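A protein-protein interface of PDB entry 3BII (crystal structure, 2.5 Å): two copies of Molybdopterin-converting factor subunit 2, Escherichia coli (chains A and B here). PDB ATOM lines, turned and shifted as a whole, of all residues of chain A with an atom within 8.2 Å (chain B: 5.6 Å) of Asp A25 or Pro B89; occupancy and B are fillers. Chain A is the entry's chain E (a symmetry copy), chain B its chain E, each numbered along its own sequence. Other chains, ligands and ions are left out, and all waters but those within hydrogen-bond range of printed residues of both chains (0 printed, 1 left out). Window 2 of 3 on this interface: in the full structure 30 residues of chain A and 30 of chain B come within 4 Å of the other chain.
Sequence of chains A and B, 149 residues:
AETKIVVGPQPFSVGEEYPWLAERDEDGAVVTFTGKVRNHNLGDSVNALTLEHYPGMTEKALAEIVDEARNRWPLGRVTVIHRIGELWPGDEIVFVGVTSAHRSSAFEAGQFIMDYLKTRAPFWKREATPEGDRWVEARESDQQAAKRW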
ATOM      1  N   LEU A  21      21.228  -4.684  -2.405  1.00  0.00           N
ATOM      2  CA  LEU A  21      20.687  -6.038  -2.390  1.00  0.00           C
ATOM      3  C   LEU A  21      20.433  -6.536  -0.963  1.00  0.00           C
ATOM      4  O   LEU A  21      19.392  -7.128  -0.695  1.00  0.00           O
ATOM      5  CB  LEU A  21      21.598  -7.001  -3.166  1.00  0.00           C
ATOM      6  CG  LEU A  21      21.150  -8.458  -3.383  1.00  0.00           C
ATOM      7  CD1 LEU A  21      19.958  -8.579  -4.363  1.00  0.00           C
ATOM      8  CD2 LEU A  21      22.347  -9.326  -3.840  1.00  0.00           C
ATOM      9  N   ALA A  22      21.350  -6.221  -0.044  1.00  0.00           N
ATOM     10  CA  ALA A  22      21.417  -6.843   1.296  1.00  0.00           C
ATOM     11  C   ALA A  22      20.797  -5.994   2.410  1.00  0.00           C
ATOM     12  O   ALA A  22      20.874  -6.325   3.595  1.00  0.00           O
ATOM     13  CB  ALA A  22      22.883  -7.171   1.629  1.00  0.00           C
ATOM     14  N   GLU A  23      20.151  -4.909   2.026  1.00  0.00           N
ATOM     15  CA  GLU A  23      19.785  -3.881   2.968  1.00  0.00           C
ATOM     16  C   GLU A  23      18.562  -4.197   3.853  1.00  0.00           C
ATOM     17  O   GLU A  23      18.518  -3.756   5.009  1.00  0.00           O
ATOM     18  CB  GLU A  23      19.567  -2.585   2.202  1.00  0.00           C
ATOM     19  CG  GLU A  23      19.293  -1.391   3.059  1.00  0.00           C
ATOM     20  CD  GLU A  23      18.719  -0.238   2.271  1.00  0.00           C
ATOM     21  OE1 GLU A  23      18.594   0.830   2.868  1.00  0.00           O
ATOM     22  OE2 GLU A  23      18.395  -0.370   1.071  1.00  0.00           O
ATOM     23  N   ARG A  24      17.568  -4.920   3.340  1.00  0.00           N
ATOM     24  CA  ARG A  24      16.408  -5.209   4.186  1.00  0.00           C
ATOM     25  C   ARG A  24      16.740  -6.312   5.193  1.00  0.00           C
ATOM     26  O   ARG A  24      17.204  -7.391   4.807  1.00  0.00           O
ATOM     27  CB  ARG A  24      15.163  -5.595   3.381  1.00  0.00           C
ATOM     28  CG  ARG A  24      14.743  -4.630   2.271  1.00  0.00           C
ATOM     29  CD  ARG A  24      13.388  -5.038   1.689  1.00  0.00           C
ATOM     30  NE  ARG A  24      13.303  -6.474   1.442  1.00  0.00           N
ATOM     31  CZ  ARG A  24      12.156  -7.138   1.302  1.00  0.00           C
ATOM     32  NH1 ARG A  24      11.014  -6.476   1.412  1.00  0.00           N
ATOM     33  NH2 ARG A  24      12.142  -8.460   1.063  1.00  0.00           N
ATOM     34  N   ASP A  25      16.503  -6.026   6.473  1.00  0.00           N
ATOM     35  CA  ASP A  25      16.679  -6.991   7.558  1.00  0.00           C
ATOM     36  C   ASP A  25      15.952  -8.320   7.354  1.00  0.00           C
ATOM     37  O   ASP A  25      16.494  -9.364   7.701  1.00  0.00           O
ATOM     38  CB  ASP A  25      16.216  -6.403   8.896  1.00  0.00           C
ATOM     39  CG  ASP A  25      17.038  -5.208   9.346  1.00  0.00           C
ATOM     40  OD1 ASP A  25      18.065  -4.843   8.712  1.00  0.00           O
ATOM     41  OD2 ASP A  25      16.638  -4.623  10.365  1.00  0.00           O
ATOM     42  N   GLU A  26      14.725  -8.290   6.832  1.00  0.00           N
ATOM     43  CA  GLU A  26      13.929  -9.528   6.715  1.00  0.00           C
ATOM     44  C   GLU A  26      14.521 -10.499   5.695  1.00  0.00           C
ATOM     45  O   GLU A  26      14.225 -11.688   5.713  1.00  0.00           O
ATOM     46  CB  GLU A  26      12.449  -9.239   6.383  1.00  0.00           C
ATOM     47  CG  GLU A  26      12.186  -8.661   4.989  1.00  0.00           C
ATOM     48  CD  GLU A  26      11.801  -7.180   5.011  1.00  0.00           C
ATOM     49  OE1 GLU A  26      12.546  -6.349   5.602  1.00  0.00           O
ATOM     50  OE2 GLU A  26      10.737  -6.849   4.424  1.00  0.00           O
ATOM     51  N   ASP A  27      15.343  -9.962   4.797  1.00  0.00           N
ATOM     52  CA  ASP A  27      16.095 -10.741   3.818  1.00  0.00           C
ATOM     53  C   ASP A  27      17.423 -11.141   4.461  1.00  0.00           C
ATOM     54  O   ASP A  27      18.453 -10.497   4.252  1.00  0.00           O
ATOM     55  CB  ASP A  27      16.362  -9.912   2.549  1.00  0.00           C
ATOM     56  CG  ASP A  27      15.081  -9.349   1.906  1.00  0.00           C
ATOM     57  OD1 ASP A  27      13.957  -9.907   2.108  1.00  0.00           O
ATOM     58  OD2 ASP A  27      15.230  -8.330   1.181  1.00  0.00           O
ATOM     59  N   GLY A  28      17.397 -12.216   5.231  1.00  0.00           N
ATOM     60  CA  GLY A  28      18.550 -12.617   6.012  1.00  0.00           C
ATOM     61  C   GLY A  28      19.538 -13.508   5.291  1.00  0.00           C
ATOM     62  O   GLY A  28      20.589 -13.818   5.857  1.00  0.00           O
ATOM     63  N   ALA A  29      19.208 -13.940   4.071  1.00  0.00           N
ATOM     64  CA  ALA A  29      20.115 -14.762   3.272  1.00  0.00           C
ATOM     65  C   ALA A  29      20.374 -14.081   1.927  1.00  0.00           C
ATOM     66  O   ALA A  29      19.455 -13.882   1.152  1.00  0.00           O
ATOM     67  CB  ALA A  29      19.549 -16.157   3.067  1.00  0.00           C
ATOM     68  N   ARG A  77      14.678  -8.610  -2.259  1.00  0.00           N
ATOM     69  CA  ARG A  77      15.265  -7.880  -3.384  1.00  0.00           C
ATOM     70  C   ARG A  77      16.100  -8.778  -4.281  1.00  0.00           C
ATOM     71  O   ARG A  77      16.782  -9.720  -3.806  1.00  0.00           O
ATOM     72  CB  ARG A  77      16.129  -6.735  -2.888  1.00  0.00           C
ATOM     73  CG  ARG A  77      15.350  -5.646  -2.194  1.00  0.00           C
ATOM     74  CD  ARG A  77      16.300  -4.607  -1.654  1.00  0.00           C
ATOM     75  NE  ARG A  77      15.595  -3.361  -1.380  1.00  0.00           N
ATOM     76  CZ  ARG A  77      16.159  -2.290  -0.831  1.00  0.00           C
ATOM     77  NH1 ARG A  77      17.437  -2.290  -0.486  1.00  0.00           N
ATOM     78  NH2 ARG A  77      15.436  -1.209  -0.625  1.00  0.00           N
ATOM     79  N   SER A 100      16.475 -13.786   0.390  1.00  0.00           N
ATOM     80  CA  SER A 100      15.361 -14.553   0.894  1.00  0.00           C
ATOM     81  C   SER A 100      15.593 -14.745   2.373  1.00  0.00           C
ATOM     82  O   SER A 100      16.650 -14.414   2.881  1.00  0.00           O
ATOM     83  CB  SER A 100      15.338 -15.903   0.177  1.00  0.00           C
ATOM     84  OG  SER A 100      14.208 -16.681   0.503  1.00  0.00           O
ATOM     85  N   ALA A 101      14.591 -15.263   3.071  1.00  0.00           N
ATOM     86  CA  ALA A 101      14.700 -15.510   4.519  1.00  0.00           C
ATOM     87  C   ALA A 101      15.618 -16.695   4.836  1.00  0.00           C
ATOM     88  O   ALA A 101      16.271 -16.707   5.875  1.00  0.00           O
ATOM     89  CB  ALA A 101      13.352 -15.734   5.115  1.00  0.00           C
ATOM     90  N   LYS B  36      22.756 -13.326   7.679  1.00  0.00           N
ATOM     91  CA  LYS B  36      22.560 -12.298   8.689  1.00  0.00           C
ATOM     92  C   LYS B  36      21.778 -12.845   9.896  1.00  0.00           C
ATOM     93  O   LYS B  36      21.166 -13.923   9.812  1.00  0.00           O
ATOM     94  CB  LYS B  36      21.826 -11.105   8.060  1.00  0.00           C
ATOM     95  CG  LYS B  36      22.640 -10.417   6.982  1.00  0.00           C
ATOM     96  CD  LYS B  36      21.766  -9.888   5.848  1.00  0.00           C
ATOM     97  CE  LYS B  36      20.735  -8.894   6.344  1.00  0.00           C
ATOM     98  NZ  LYS B  36      19.974  -8.290   5.206  1.00  0.00           N
ATOM     99  N   VAL B  37      21.807 -12.085  10.996  1.00  0.00           N
ATOM    100  CA  VAL B  37      21.020 -12.362  12.200  1.00  0.00           C
ATOM    101  C   VAL B  37      19.528 -12.168  11.933  1.00  0.00           C
ATOM    102  O   VAL B  37      19.119 -11.113  11.435  1.00  0.00           O
ATOM    103  CB  VAL B  37      21.420 -11.408  13.349  1.00  0.00           C
ATOM    104  CG1 VAL B  37      20.583 -11.678  14.608  1.00  0.00           C
ATOM    105  CG2 VAL B  37      22.911 -11.499  13.641  1.00  0.00           C
ATOM    106  N   ARG B  38      18.723 -13.171  12.293  1.00  0.00           N
ATOM    107  CA  ARG B  38      17.259 -13.137  12.076  1.00  0.00           C
ATOM    108  C   ARG B  38      16.535 -12.541  13.300  1.00  0.00           C
ATOM    109  O   ARG B  38      16.971 -12.747  14.445  1.00  0.00           O
ATOM    110  CB  ARG B  38      16.724 -14.553  11.794  1.00  0.00           C
ATOM    111  CG  ARG B  38      17.653 -15.460  10.947  1.00  0.00           C
ATOM    112  CD  ARG B  38      18.029 -14.837   9.560  1.00  0.00           C
ATOM    113  NE  ARG B  38      17.899 -15.813   8.460  1.00  0.00           N
ATOM    114  CZ  ARG B  38      18.910 -16.403   7.802  1.00  0.00           C
ATOM    115  NH1 ARG B  38      20.206 -16.130   8.066  1.00  0.00           N
ATOM    116  NH2 ARG B  38      18.618 -17.269   6.846  1.00  0.00           N
ATOM    117  N   VAL B  46      12.502  -7.394  18.874  1.00  0.00           N
ATOM    118  CA  VAL B  46      13.890  -7.328  18.393  1.00  0.00           C
ATOM    119  C   VAL B  46      14.935  -7.550  19.505  1.00  0.00           C
ATOM    120  O   VAL B  46      15.038  -6.743  20.422  1.00  0.00           O
ATOM    121  CB  VAL B  46      14.160  -6.003  17.642  1.00  0.00           C
ATOM    122  CG1 VAL B  46      15.652  -5.704  17.564  1.00  0.00           C
ATOM    123  CG2 VAL B  46      13.578  -6.069  16.248  1.00  0.00           C
ATOM    124  N   ASN B  47      15.712  -8.638  19.402  1.00  0.00           N
ATOM    125  CA  ASN B  47      16.729  -9.038  20.437  1.00  0.00           C
ATOM    126  C   ASN B  47      18.165  -9.248  19.949  1.00  0.00           C
ATOM    127  O   ASN B  47      18.395  -9.803  18.901  1.00  0.00           O
ATOM    128  CB  ASN B  47      16.286 -10.312  21.182  1.00  0.00           C
ATOM    129  CG  ASN B  47      14.887 -10.197  21.743  1.00  0.00           C
ATOM    130  OD1 ASN B  47      14.102 -11.154  21.695  1.00  0.00           O
ATOM    131  ND2 ASN B  47      14.555  -9.008  22.269  1.00  0.00           N
ATOM    132  N   ALA B  48      19.123  -8.811  20.745  1.00  0.00           N
ATOM    133  CA  ALA B  48      20.536  -9.063  20.482  1.00  0.00           C
ATOM    134  C   ALA B  48      20.832 -10.564  20.504  1.00  0.00           C
ATOM    135  O   ALA B  48      20.199 -11.316  21.251  1.00  0.00           O
ATOM    136  CB  ALA B  48      21.405  -8.332  21.532  1.00  0.00           C
ATOM    137  N   LEU B  87      25.455  -9.424  18.243  1.00  0.00           N
ATOM    138  CA  LEU B  87      25.032  -8.862  16.975  1.00  0.00           C
ATOM    139  C   LEU B  87      23.547  -8.691  17.074  1.00  0.00           C
ATOM    140  O   LEU B  87      22.938  -9.193  18.030  1.00  0.00           O
ATOM    141  CB  LEU B  87      25.393  -9.788  15.814  1.00  0.00           C
ATOM    142  CG  LEU B  87      26.882 -10.054  15.615  1.00  0.00           C
ATOM    143  CD1 LEU B  87      27.107 -11.302  14.766  1.00  0.00           C
ATOM    144  CD2 LEU B  87      27.574  -8.809  15.043  1.00  0.00           C
ATOM    145  N   TRP B  88      22.973  -7.975  16.104  1.00  0.00           N
ATOM    146  CA  TRP B  88      21.541  -7.654  16.101  1.00  0.00           C
ATOM    147  C   TRP B  88      20.956  -8.020  14.753  1.00  0.00           C
ATOM    148  O   TRP B  88      21.699  -8.083  13.781  1.00  0.00           O
ATOM    149  CB  TRP B  88      21.349  -6.160  16.357  1.00  0.00           C
ATOM    150  CG  TRP B  88      21.749  -5.734  17.715  1.00  0.00           C
ATOM    151  CD1 TRP B  88      23.023  -5.515  18.173  1.00  0.00           C
ATOM    152  CD2 TRP B  88      20.865  -5.445  18.808  1.00  0.00           C
ATOM    153  NE1 TRP B  88      22.983  -5.127  19.503  1.00  0.00           N
ATOM    154  CE2 TRP B  88      21.672  -5.074  19.911  1.00  0.00           C
ATOM    155  CE3 TRP B  88      19.471  -5.466  18.958  1.00  0.00           C
ATOM    156  CZ2 TRP B  88      21.130  -4.729  21.146  1.00  0.00           C
ATOM    157  CZ3 TRP B  88      18.931  -5.133  20.172  1.00  0.00           C
ATOM    158  CH2 TRP B  88      19.761  -4.768  21.263  1.00  0.00           C
ATOM    159  N   PRO B  89      19.630  -8.245  14.683  1.00  0.00           N
ATOM    160  CA  PRO B  89      18.973  -8.582  13.397  1.00  0.00           C
ATOM    161  C   PRO B  89      19.358  -7.612  12.306  1.00  0.00           C
ATOM    162  O   PRO B  89      19.301  -6.395  12.519  1.00  0.00           O
ATOM    163  CB  PRO B  89      17.461  -8.493  13.705  1.00  0.00           C
ATOM    164  CG  PRO B  89      17.353  -8.692  15.167  1.00  0.00           C
ATOM    165  CD  PRO B  89      18.674  -8.227  15.808  1.00  0.00           C
ATOM    166  N   GLY B  90      19.796  -8.142  11.163  1.00  0.00           N
ATOM    167  CA  GLY B  90      20.266  -7.303  10.040  1.00  0.00           C
ATOM    168  C   GLY B  90      21.780  -7.196   9.938  1.00  0.00           C
ATOM    169  O   GLY B  90      22.313  -6.802   8.893  1.00  0.00           O
ATOM    170  N   ASP B  91      22.490  -7.521  11.017  1.00  0.00           N
ATOM    171  CA  ASP B  91      23.950  -7.611  10.949  1.00  0.00           C
ATOM    172  C   ASP B  91      24.353  -8.874  10.185  1.00  0.00           C
ATOM    173  O   ASP B  91      23.751  -9.949  10.341  1.00  0.00           O
ATOM    174  CB  ASP B  91      24.568  -7.643  12.333  1.00  0.00           C
ATOM    175  CG  ASP B  91      24.206  -6.437  13.163  1.00  0.00           C
ATOM    176  OD1 ASP B  91      23.545  -5.511  12.626  1.00  0.00           O
ATOM    177  OD2 ASP B  91      24.581  -6.420  14.367  1.00  0.00           O
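The backbone carbonyl oxygen of Ala A101 is in hydrogen-bond range of the guanidinium group of Arg B38 (2.6 Å). O of Gly A28 sits at hydrogen-bond distance from N of Lys B36, at 2.9 Å. The side-chain amino group (NZ) of Lys B36 lies within hydrogen-bond range of the backbone carbonyl oxygen (O) of Arg A24 (2.9 Å). NH1 of Arg B38 is in hydrogen-bond range of O of Gly A28 (3.2 Å). The side-chain amino group (NZ) of Lys B36 is in hydrogen-bond range of the backbone carbonyl oxygen (O) of Asp A27, 2.8 Å away. NZ of Lys B36 is in hydrogen-bond range of O of Ala A22 (2.7 Å).
Among the printed residues, pairs that only touch across the chains: Asp A25 with Gly B90 and Asp A25 with Pro B89.
Of the 12 printed residues of chain A, 6 touch a printed residue of chain B. Of the 11 printed residues of chain B, 4 touch a printed residue of chain A. Among the printed residues, no Asp or Glu carboxylate lies within 4 Å of a Lys or Arg side-chain nitrogen of the other chain.
No position is printed for both chains. Of the 8 pairs that touch across the chains among the printed residues, none has its exchanged pair printed and touching as well.
N of Gly B90 is in hydrogen-bond range of O of Val B37, at 3.1 Å. The guanidinium group (NH2) of Arg A24 lies within salt-bridge range of the side-chain carboxylate (OD1) of Asp A27 (2.5 Å). The backbone NH (N) of Arg A77 lies within hydrogen-bond range of the side-chain carboxylate (OD2) of Asp A27 (3.5 Å). The backbone carbonyl oxygen (O) of Lys B36 is in hydrogen-bond range of the guanidinium group (NH1) of Arg B38 (3.0 Å). NH1 of Arg A24 is in salt-bridge range of OE2 of Glu A26. The backbone NH (N) of Gly A28 sits at hydrogen-bond distance from the backbone carbonyl oxygen (O) of Ser A100 (3.3 Å).
Asp A25 touches just these residues of chain B: Pro B89 and Gly B90. Pro B89 touches just one residue of chain A: Asp A25. Printed residues of chain B within 4 Å of Ala A22: Lys B36. Printed residues of chain A within 4 Å of Lys B36: Ala A22, Arg A24, Asp A27 and Gly A28. Printed residues of chain B within 4 Å of Asp A27: Lys B36. Asn B47 touches none of the printed residues of chain A. Ala B48 touches none of the printed residues of chain A. The nearest residue of chain A that does not touch Pro B89 is Glu A26 (7.2 Å). The nearest printed residue of chain B that does not touch Arg A24 is Gly B90 (6.1 Å).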
